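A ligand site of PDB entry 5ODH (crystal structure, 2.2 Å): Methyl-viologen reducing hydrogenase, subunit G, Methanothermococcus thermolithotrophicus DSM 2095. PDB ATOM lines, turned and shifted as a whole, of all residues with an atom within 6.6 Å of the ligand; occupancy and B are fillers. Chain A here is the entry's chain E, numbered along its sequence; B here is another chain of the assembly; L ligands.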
ATOM      1  N   GLY A  10     -27.334 -19.196  -9.317  1.00  0.00           N
ATOM      2  CA  GLY A  10     -28.080 -17.960  -9.254  1.00  0.00           C
ATOM      3  C   GLY A  10     -27.838 -17.178  -7.986  1.00  0.00           C
ATOM      4  O   GLY A  10     -28.727 -16.467  -7.520  1.00  0.00           O
ATOM      5  N   GLY A  11     -26.647 -17.313  -7.402  1.00  0.00           N
ATOM      6  CA  GLY A  11     -26.279 -16.600  -6.204  1.00  0.00           C
ATOM      7  C   GLY A  11     -25.489 -15.339  -6.507  1.00  0.00           C
ATOM      8  O   GLY A  11     -25.455 -14.836  -7.633  1.00  0.00           O
ATOM      9  N   CYS A  12     -24.858 -14.804  -5.461  1.00  0.00           N
ATOM     10  CA  CYS A  12     -24.085 -13.570  -5.580  1.00  0.00           C
ATOM     11  C   CYS A  12     -22.612 -13.753  -5.201  1.00  0.00           C
ATOM     12  O   CYS A  12     -21.881 -12.759  -5.120  1.00  0.00           O
ATOM     13  CB  CYS A  12     -24.711 -12.478  -4.721  1.00  0.00           C
ATOM     14  SG  CYS A  12     -24.168 -12.449  -3.009  1.00  0.00           S
ATOM     15  N   SER A  13     -22.168 -14.990  -4.986  1.00  0.00           N
ATOM     16  CA  SER A  13     -20.805 -15.353  -4.577  1.00  0.00           C
ATOM     17  C   SER A  13     -20.585 -15.224  -3.073  1.00  0.00           C
ATOM     18  O   SER A  13     -19.506 -15.586  -2.591  1.00  0.00           O
ATOM     19  CB  SER A  13     -19.728 -14.516  -5.276  1.00  0.00           C
ATOM     20  OG  SER A  13     -19.648 -13.223  -4.704  1.00  0.00           O
ATOM     21  N   GLY A  14     -21.576 -14.757  -2.318  1.00  0.00           N
ATOM     22  CA  GLY A  14     -21.381 -14.532  -0.887  1.00  0.00           C
ATOM     23  C   GLY A  14     -21.010 -15.784  -0.127  1.00  0.00           C
ATOM     24  O   GLY A  14     -20.253 -15.718   0.848  1.00  0.00           O
ATOM     25  N   CYS A  15     -21.526 -16.938  -0.540  1.00  0.00           N
ATOM     26  CA  CYS A  15     -21.142 -18.185   0.113  1.00  0.00           C
ATOM     27  C   CYS A  15     -19.650 -18.448  -0.035  1.00  0.00           C
ATOM     28  O   CYS A  15     -18.986 -18.853   0.920  1.00  0.00           O
ATOM     29  CB  CYS A  15     -21.935 -19.360  -0.451  1.00  0.00           C
ATOM     30  SG  CYS A  15     -23.625 -19.460   0.096  1.00  0.00           S
ATOM     31  N   HIS A  16     -19.116 -18.216  -1.227  1.00  0.00           N
ATOM     32  CA  HIS A  16     -17.684 -18.413  -1.441  1.00  0.00           C
ATOM     33  C   HIS A  16     -16.871 -17.442  -0.598  1.00  0.00           C
ATOM     34  O   HIS A  16     -15.834 -17.819  -0.029  1.00  0.00           O
ATOM     35  CB  HIS A  16     -17.347 -18.251  -2.921  1.00  0.00           C
ATOM     36  CG  HIS A  16     -17.700 -19.448  -3.742  1.00  0.00           C
ATOM     37  ND1 HIS A  16     -18.998 -19.833  -3.989  1.00  0.00           N
ATOM     38  CD2 HIS A  16     -16.913 -20.353  -4.371  1.00  0.00           C
ATOM     39  CE1 HIS A  16     -18.996 -20.914  -4.748  1.00  0.00           C
ATOM     40  NE2 HIS A  16     -17.745 -21.255  -4.989  1.00  0.00           N
ATOM     41  N   GLU A  57     -23.404 -23.310  -4.810  1.00  0.00           N
ATOM     42  CA  GLU A  57     -23.998 -22.067  -4.353  1.00  0.00           C
ATOM     43  C   GLU A  57     -25.082 -21.623  -5.328  1.00  0.00           C
ATOM     44  O   GLU A  57     -25.014 -21.908  -6.528  1.00  0.00           O
ATOM     45  CB  GLU A  57     -22.927 -20.974  -4.218  1.00  0.00           C
ATOM     46  CG  GLU A  57     -23.458 -19.557  -3.991  1.00  0.00           C
ATOM     47  CD  GLU A  57     -22.416 -18.492  -4.321  1.00  0.00           C
ATOM     48  OE1 GLU A  57     -22.546 -17.838  -5.377  1.00  0.00           O
ATOM     49  OE2 GLU A  57     -21.462 -18.331  -3.531  1.00  0.00           O
ATOM     50  N   GLY A  58     -26.095 -20.941  -4.796  1.00  0.00           N
ATOM     51  CA  GLY A  58     -27.103 -20.301  -5.625  1.00  0.00           C
ATOM     52  C   GLY A  58     -28.205 -21.227  -6.098  1.00  0.00           C
ATOM     53  O   GLY A  58     -27.986 -22.426  -6.263  1.00  0.00           O
ATOM     54  N   GLY A  59     -29.382 -20.661  -6.346  1.00  0.00           N
ATOM     55  CA  GLY A  59     -30.491 -21.424  -6.879  1.00  0.00           C
ATOM     56  C   GLY A  59     -30.435 -21.519  -8.400  1.00  0.00           C
ATOM     57  O   GLY A  59     -29.476 -21.110  -9.050  1.00  0.00           O
ATOM     58  N   PHE A  82     -25.328 -25.129  -0.964  1.00  0.00           N
ATOM     59  CA  PHE A  82     -24.471 -24.222  -0.223  1.00  0.00           C
ATOM     60  C   PHE A  82     -25.150 -22.864  -0.113  1.00  0.00           C
ATOM     61  O   PHE A  82     -25.113 -22.054  -1.045  1.00  0.00           O
ATOM     62  CB  PHE A  82     -23.116 -24.115  -0.916  1.00  0.00           C
ATOM     63  CG  PHE A  82     -22.065 -23.377  -0.122  1.00  0.00           C
ATOM     64  CD1 PHE A  82     -22.257 -23.045   1.208  1.00  0.00           C
ATOM     65  CD2 PHE A  82     -20.872 -23.017  -0.734  1.00  0.00           C
ATOM     66  CE1 PHE A  82     -21.295 -22.372   1.916  1.00  0.00           C
ATOM     67  CE2 PHE A  82     -19.900 -22.346  -0.029  1.00  0.00           C
ATOM     68  CZ  PHE A  82     -20.105 -22.017   1.296  1.00  0.00           C
ATOM     69  N   GLY A  83     -25.778 -22.609   1.027  1.00  0.00           N
ATOM     70  CA  GLY A  83     -26.390 -21.328   1.319  1.00  0.00           C
ATOM     71  C   GLY A  83     -27.871 -21.291   1.008  1.00  0.00           C
ATOM     72  O   GLY A  83     -28.443 -22.193   0.376  1.00  0.00           O
ATOM     73  N   THR A  84     -28.478 -20.186   1.432  1.00  0.00           N
ATOM     74  CA  THR A  84     -29.928 -20.042   1.389  1.00  0.00           C
ATOM     75  C   THR A  84     -30.479 -20.034  -0.033  1.00  0.00           C
ATOM     76  O   THR A  84     -31.547 -20.599  -0.283  1.00  0.00           O
ATOM     77  CB  THR A  84     -30.330 -18.748   2.124  1.00  0.00           C
ATOM     78  OG1 THR A  84     -30.128 -18.922   3.537  1.00  0.00           O
ATOM     79  CG2 THR A  84     -31.783 -18.417   1.869  1.00  0.00           C
ATOM     80  N   CYS A  85     -29.775 -19.418  -0.982  1.00  0.00           N
ATOM     81  CA  CYS A  85     -30.269 -19.404  -2.357  1.00  0.00           C
ATOM     82  C   CYS A  85     -30.395 -20.828  -2.892  1.00  0.00           C
ATOM     83  O   CYS A  85     -31.444 -21.222  -3.416  1.00  0.00           O
ATOM     84  CB  CYS A  85     -29.359 -18.579  -3.268  1.00  0.00           C
ATOM     85  SG  CYS A  85     -29.670 -16.792  -3.255  1.00  0.00           S
ATOM     86  N   ALA A  86     -29.336 -21.614  -2.736  1.00  0.00           N
ATOM     87  CA  ALA A  86     -29.363 -22.992  -3.214  1.00  0.00           C
ATOM     88  C   ALA A  86     -30.371 -23.836  -2.451  1.00  0.00           C
ATOM     89  O   ALA A  86     -30.963 -24.761  -3.025  1.00  0.00           O
ATOM     90  CB  ALA A  86     -27.974 -23.608  -3.118  1.00  0.00           C
ATOM     91  N   GLY A  89     -33.904 -20.741  -2.344  1.00  0.00           N
ATOM     92  CA  GLY A  89     -34.130 -19.862  -3.476  1.00  0.00           C
ATOM     93  C   GLY A  89     -33.545 -18.473  -3.272  1.00  0.00           C
ATOM     94  O   GLY A  89     -33.041 -17.862  -4.214  1.00  0.00           O
ATOM     95  N   GLY A  90     -33.615 -17.965  -2.035  1.00  0.00           N
ATOM     96  CA  GLY A  90     -32.955 -16.726  -1.693  1.00  0.00           C
ATOM     97  C   GLY A  90     -33.634 -15.477  -2.233  1.00  0.00           C
ATOM     98  O   GLY A  90     -34.773 -15.485  -2.687  1.00  0.00           O
ATOM     99  N   VAL A  91     -32.889 -14.378  -2.135  1.00  0.00           N
ATOM    100  CA  VAL A  91     -33.410 -13.080  -2.593  1.00  0.00           C
ATOM    101  C   VAL A  91     -33.743 -13.111  -4.076  1.00  0.00           C
ATOM    102  O   VAL A  91     -34.767 -12.530  -4.467  1.00  0.00           O
ATOM    103  CB  VAL A  91     -32.445 -11.960  -2.210  1.00  0.00           C
ATOM    104  CG1 VAL A  91     -32.762 -10.691  -2.977  1.00  0.00           C
ATOM    105  CG2 VAL A  91     -32.513 -11.707  -0.719  1.00  0.00           C
ATOM    106  N   PRO A  92     -32.948 -13.713  -4.956  1.00  0.00           N
ATOM    107  CA  PRO A  92     -33.342 -13.765  -6.379  1.00  0.00           C
ATOM    108  C   PRO A  92     -34.717 -14.364  -6.612  1.00  0.00           C
ATOM    109  O   PRO A  92     -35.326 -14.137  -7.664  1.00  0.00           O
ATOM    110  CB  PRO A  92     -32.254 -14.638  -7.008  1.00  0.00           C
ATOM    111  CG  PRO A  92     -31.105 -14.623  -6.068  1.00  0.00           C
ATOM    112  CD  PRO A  92     -31.601 -14.252  -4.718  1.00  0.00           C
ATOM    113  N   GLY A 148     -28.093 -20.296   5.480  1.00  0.00           N
ATOM    114  CA  GLY A 148     -27.414 -19.052   5.774  1.00  0.00           C
ATOM    115  C   GLY A 148     -27.219 -18.194   4.541  1.00  0.00           C
ATOM    116  O   GLY A 148     -26.894 -18.718   3.474  1.00  0.00           O
ATOM    117  N   CYS A 149     -27.390 -16.886   4.694  1.00  0.00           N
ATOM    118  CA  CYS A 149     -27.195 -15.920   3.617  1.00  0.00           C
ATOM    119  C   CYS A 149     -26.208 -14.843   4.067  1.00  0.00           C
ATOM    120  O   CYS A 149     -26.606 -13.717   4.396  1.00  0.00           O
ATOM    121  CB  CYS A 149     -28.535 -15.319   3.213  1.00  0.00           C
ATOM    122  SG  CYS A 149     -28.538 -13.731   2.301  1.00  0.00           S
ATOM    123  N   PRO A 150     -24.918 -15.197   4.128  1.00  0.00           N
ATOM    124  CA  PRO A 150     -24.326 -16.501   3.857  1.00  0.00           C
ATOM    125  C   PRO A 150     -24.205 -17.344   5.119  1.00  0.00           C
ATOM    126  O   PRO A 150     -24.385 -16.809   6.208  1.00  0.00           O
ATOM    127  CB  PRO A 150     -22.938 -16.150   3.310  1.00  0.00           C
ATOM    128  CG  PRO A 150     -22.636 -14.773   3.868  1.00  0.00           C
ATOM    129  CD  PRO A 150     -23.895 -14.227   4.518  1.00  0.00           C
ATOM    130  N   PRO A 151     -23.911 -18.633   4.980  1.00  0.00           N
ATOM    131  CA  PRO A 151     -23.574 -19.437   6.158  1.00  0.00           C
ATOM    132  C   PRO A 151     -22.280 -18.943   6.773  1.00  0.00           C
ATOM    133  O   PRO A 151     -21.297 -18.720   6.067  1.00  0.00           O
ATOM    134  CB  PRO A 151     -23.421 -20.864   5.603  1.00  0.00           C
ATOM    135  CG  PRO A 151     -23.959 -20.828   4.207  1.00  0.00           C
ATOM    136  CD  PRO A 151     -23.834 -19.421   3.727  1.00  0.00           C
ATOM    137  N   CYS A 238     -32.819 -14.898   7.135  1.00  0.00           N
ATOM    138  CA  CYS A 238     -31.949 -15.348   6.046  1.00  0.00           C
ATOM    139  C   CYS A 238     -31.589 -16.824   6.157  1.00  0.00           C
ATOM    140  O   CYS A 238     -31.341 -17.477   5.126  1.00  0.00           O
ATOM    141  CB  CYS A 238     -30.677 -14.504   6.009  1.00  0.00           C
ATOM    142  SG  CYS A 238     -29.224 -15.285   6.751  1.00  0.00           S
ATOM    143  N   PHE A 287     -36.162 -14.441   1.690  1.00  0.00           N
ATOM    144  CA  PHE A 287     -35.114 -15.369   1.295  1.00  0.00           C
ATOM    145  C   PHE A 287     -35.622 -16.737   0.861  1.00  0.00           C
ATOM    146  O   PHE A 287     -34.813 -17.548   0.402  1.00  0.00           O
ATOM    147  CB  PHE A 287     -34.129 -15.554   2.459  1.00  0.00           C
ATOM    148  CG  PHE A 287     -33.508 -14.275   2.941  1.00  0.00           C
ATOM    149  CD1 PHE A 287     -34.122 -13.523   3.917  1.00  0.00           C
ATOM    150  CD2 PHE A 287     -32.300 -13.841   2.413  1.00  0.00           C
ATOM    151  CE1 PHE A 287     -33.549 -12.337   4.363  1.00  0.00           C
ATOM    152  CE2 PHE A 287     -31.727 -12.654   2.858  1.00  0.00           C
ATOM    153  CZ  PHE A 287     -32.353 -11.905   3.829  1.00  0.00           C
ATOM    154  N   ARG B  39     -30.386 -11.464 -12.827  1.00  0.00           N
ATOM    155  CA  ARG B  39     -31.356 -11.816 -11.800  1.00  0.00           C
ATOM    156  C   ARG B  39     -32.548 -10.873 -11.704  1.00  0.00           C
ATOM    157  O   ARG B  39     -33.607 -11.315 -11.242  1.00  0.00           O
ATOM    158  CB  ARG B  39     -30.673 -11.891 -10.425  1.00  0.00           C
ATOM    159  CG  ARG B  39     -29.789 -13.127 -10.258  1.00  0.00           C
ATOM    160  CD  ARG B  39     -28.888 -13.035  -9.045  1.00  0.00           C
ATOM    161  NE  ARG B  39     -27.873 -11.995  -9.189  1.00  0.00           N
ATOM    162  CZ  ARG B  39     -27.183 -11.475  -8.183  1.00  0.00           C
ATOM    163  NH1 ARG B  39     -27.381 -11.894  -6.945  1.00  0.00           N
ATOM    164  NH2 ARG B  39     -26.294 -10.526  -8.419  1.00  0.00           N
ATOM    165  N   PRO B  58     -27.529  -5.761  -0.935  1.00  0.00           N
ATOM    166  CA  PRO B  58     -26.285  -6.504  -0.667  1.00  0.00           C
ATOM    167  C   PRO B  58     -26.251  -7.869  -1.313  1.00  0.00           C
ATOM    168  O   PRO B  58     -25.161  -8.331  -1.677  1.00  0.00           O
ATOM    169  CB  PRO B  58     -26.254  -6.580   0.864  1.00  0.00           C
ATOM    170  CG  PRO B  58     -26.993  -5.358   1.305  1.00  0.00           C
ATOM    171  CD  PRO B  58     -28.076  -5.145   0.297  1.00  0.00           C
ATOM    172  N   ARG B  59     -27.400  -8.536  -1.482  1.00  0.00           N
ATOM    173  CA  ARG B  59     -27.388  -9.843  -2.131  1.00  0.00           C
ATOM    174  C   ARG B  59     -27.162  -9.748  -3.625  1.00  0.00           C
ATOM    175  O   ARG B  59     -27.192 -10.779  -4.303  1.00  0.00           O
ATOM    176  CB  ARG B  59     -28.692 -10.596  -1.852  1.00  0.00           C
ATOM    177  CG  ARG B  59     -28.691 -11.361  -0.542  1.00  0.00           C
ATOM    178  CD  ARG B  59     -28.820 -10.413   0.645  1.00  0.00           C
ATOM    179  NE  ARG B  59     -28.479 -11.044   1.913  1.00  0.00           N
ATOM    180  CZ  ARG B  59     -28.738 -10.517   3.101  1.00  0.00           C
ATOM    181  NH1 ARG B  59     -29.352  -9.340   3.186  1.00  0.00           N
ATOM    182  NH2 ARG B  59     -28.380 -11.155   4.206  1.00  0.00           N
ATOM    183  N   CYS B  61     -24.241  -8.926  -4.539  1.00  0.00           N
ATOM    184  CA  CYS B  61     -22.898  -9.472  -4.541  1.00  0.00           C
ATOM    185  C   CYS B  61     -22.393  -9.661  -3.126  1.00  0.00           C
ATOM    186  O   CYS B  61     -22.619  -8.824  -2.254  1.00  0.00           O
ATOM    187  CB  CYS B  61     -21.931  -8.567  -5.302  1.00  0.00           C
ATOM    188  SG  CYS B  61     -20.257  -9.168  -5.177  1.00  0.00           S
ATOM    189  N   GLY B  62     -21.637 -10.741  -2.918  1.00  0.00           N
ATOM    190  CA  GLY B  62     -21.056 -11.018  -1.626  1.00  0.00           C
ATOM    191  C   GLY B  62     -19.725 -10.381  -1.350  1.00  0.00           C
ATOM    192  O   GLY B  62     -19.298 -10.335  -0.184  1.00  0.00           O
ATOM    193  N   ILE B 162     -20.426  -9.965   6.112  1.00  0.00           N
ATOM    194  CA  ILE B 162     -21.016 -10.086   4.785  1.00  0.00           C
ATOM    195  C   ILE B 162     -22.501  -9.754   4.912  1.00  0.00           C
ATOM    196  O   ILE B 162     -23.222 -10.406   5.668  1.00  0.00           O
ATOM    197  CB  ILE B 162     -20.821 -11.481   4.168  1.00  0.00           C
ATOM    198  CG1 ILE B 162     -19.331 -11.821   4.142  1.00  0.00           C
ATOM    199  CG2 ILE B 162     -21.398 -11.522   2.761  1.00  0.00           C
ATOM    200  CD1 ILE B 162     -19.010 -13.200   3.554  1.00  0.00           C
ATOM    201  N   HIS B 163     -22.937  -8.722   4.176  1.00  0.00           N
ATOM    202  CA  HIS B 163     -24.270  -8.169   4.245  1.00  0.00           C
ATOM    203  C   HIS B 163     -24.466  -7.450   5.574  1.00  0.00           C
ATOM    204  O   HIS B 163     -25.140  -7.961   6.484  1.00  0.00           O
ATOM    205  CB  HIS B 163     -25.322  -9.266   4.030  1.00  0.00           C
ATOM    206  CG  HIS B 163     -25.139 -10.014   2.749  1.00  0.00           C
ATOM    207  ND1 HIS B 163     -24.817  -9.398   1.565  1.00  0.00           N
ATOM    208  CD2 HIS B 163     -25.227 -11.337   2.471  1.00  0.00           C
ATOM    209  CE1 HIS B 163     -24.698 -10.296   0.611  1.00  0.00           C
ATOM    210  NE2 HIS B 163     -24.952 -11.487   1.132  1.00  0.00           N
HETATM  211 FE1  LIG L   1     -24.930 -17.244  -0.225  1.00  0.00          FE
HETATM  212 FE2  LIG L   1     -25.081 -14.562  -1.900  1.00  0.00          FE
HETATM  213 FE3  LIG L   1     -27.108 -15.009   0.587  1.00  0.00          FE
HETATM  214 FE4  LIG L   1     -27.414 -16.635  -2.178  1.00  0.00          FE
HETATM  215  S1  LIG L   1     -27.109 -14.702  -1.481  1.00  0.00           S
HETATM  216  S2  LIG L   1     -26.996 -16.943  -0.160  1.00  0.00           S
HETATM  217  S3  LIG L   1     -25.339 -16.596  -2.170  1.00  0.00           S
HETATM  218  S4  LIG L   1     -25.099 -15.207   0.098  1.00  0.00           S
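Gly 14 touches the ligand (N to FE2, 3.5 Å). Glu 57 touches the ligand. Thr 84 touches the ligand (N to S2, 3.9 Å). CB of Pro 150 touches S4 of the ligand, at 3.98 Å. Arg 59 of chain B touches the ligand (CG to S1, 3.8 Å). His 163 of chain B touches the ligand. Hydrophobic or aromatic side chains within 4 Å of the ligand: Pro 150. The nearest printed residue that does not touch the ligand is Gly 148 (4.05 Å).
FE3 of the ligand is bound by SG of Cys 149, at 2.6 Å. FE4 of the ligand is bound by SG of Cys 85 (2.5 Å). The side-chain sulfur (SG) of Cys 12 is bound to an iron atom (FE2) of the ligand (2.6 Å). FE1 of the ligand is bound by SG of Cys 15 (2.6 Å). The backbone NH (N) of Cys 12 lies close to a sulfur (S3) of the ligand, 3.8 Å away.
The backbone NH of Gly 14 sits close to the side-chain sulfur of Cys 12 (3.5 Å). The backbone NH of Thr 84 is in hydrogen-bond range of the backbone carbonyl oxygen of Gly 148, 3.0 Å away. OE2 of Glu 57 sits at hydrogen-bond distance from ND1 of His 16 (2.9 Å). N of Ser 13 sits at hydrogen-bond distance from OE1 of Glu 57. O of Pro 58 of chain B lies close to ND1 of His 163 of chain B (3.4 Å). O of Cys 12 lies within hydrogen-bond range of N of Gly 62 of chain B (3.0 Å). NH1 of Arg 39 of chain B sits at hydrogen-bond distance from O of Arg 59 of chain B. The backbone NH (N) of Gly 89 is in hydrogen-bond range of the backbone carbonyl oxygen (O) of Thr 84, 3.1 Å away.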
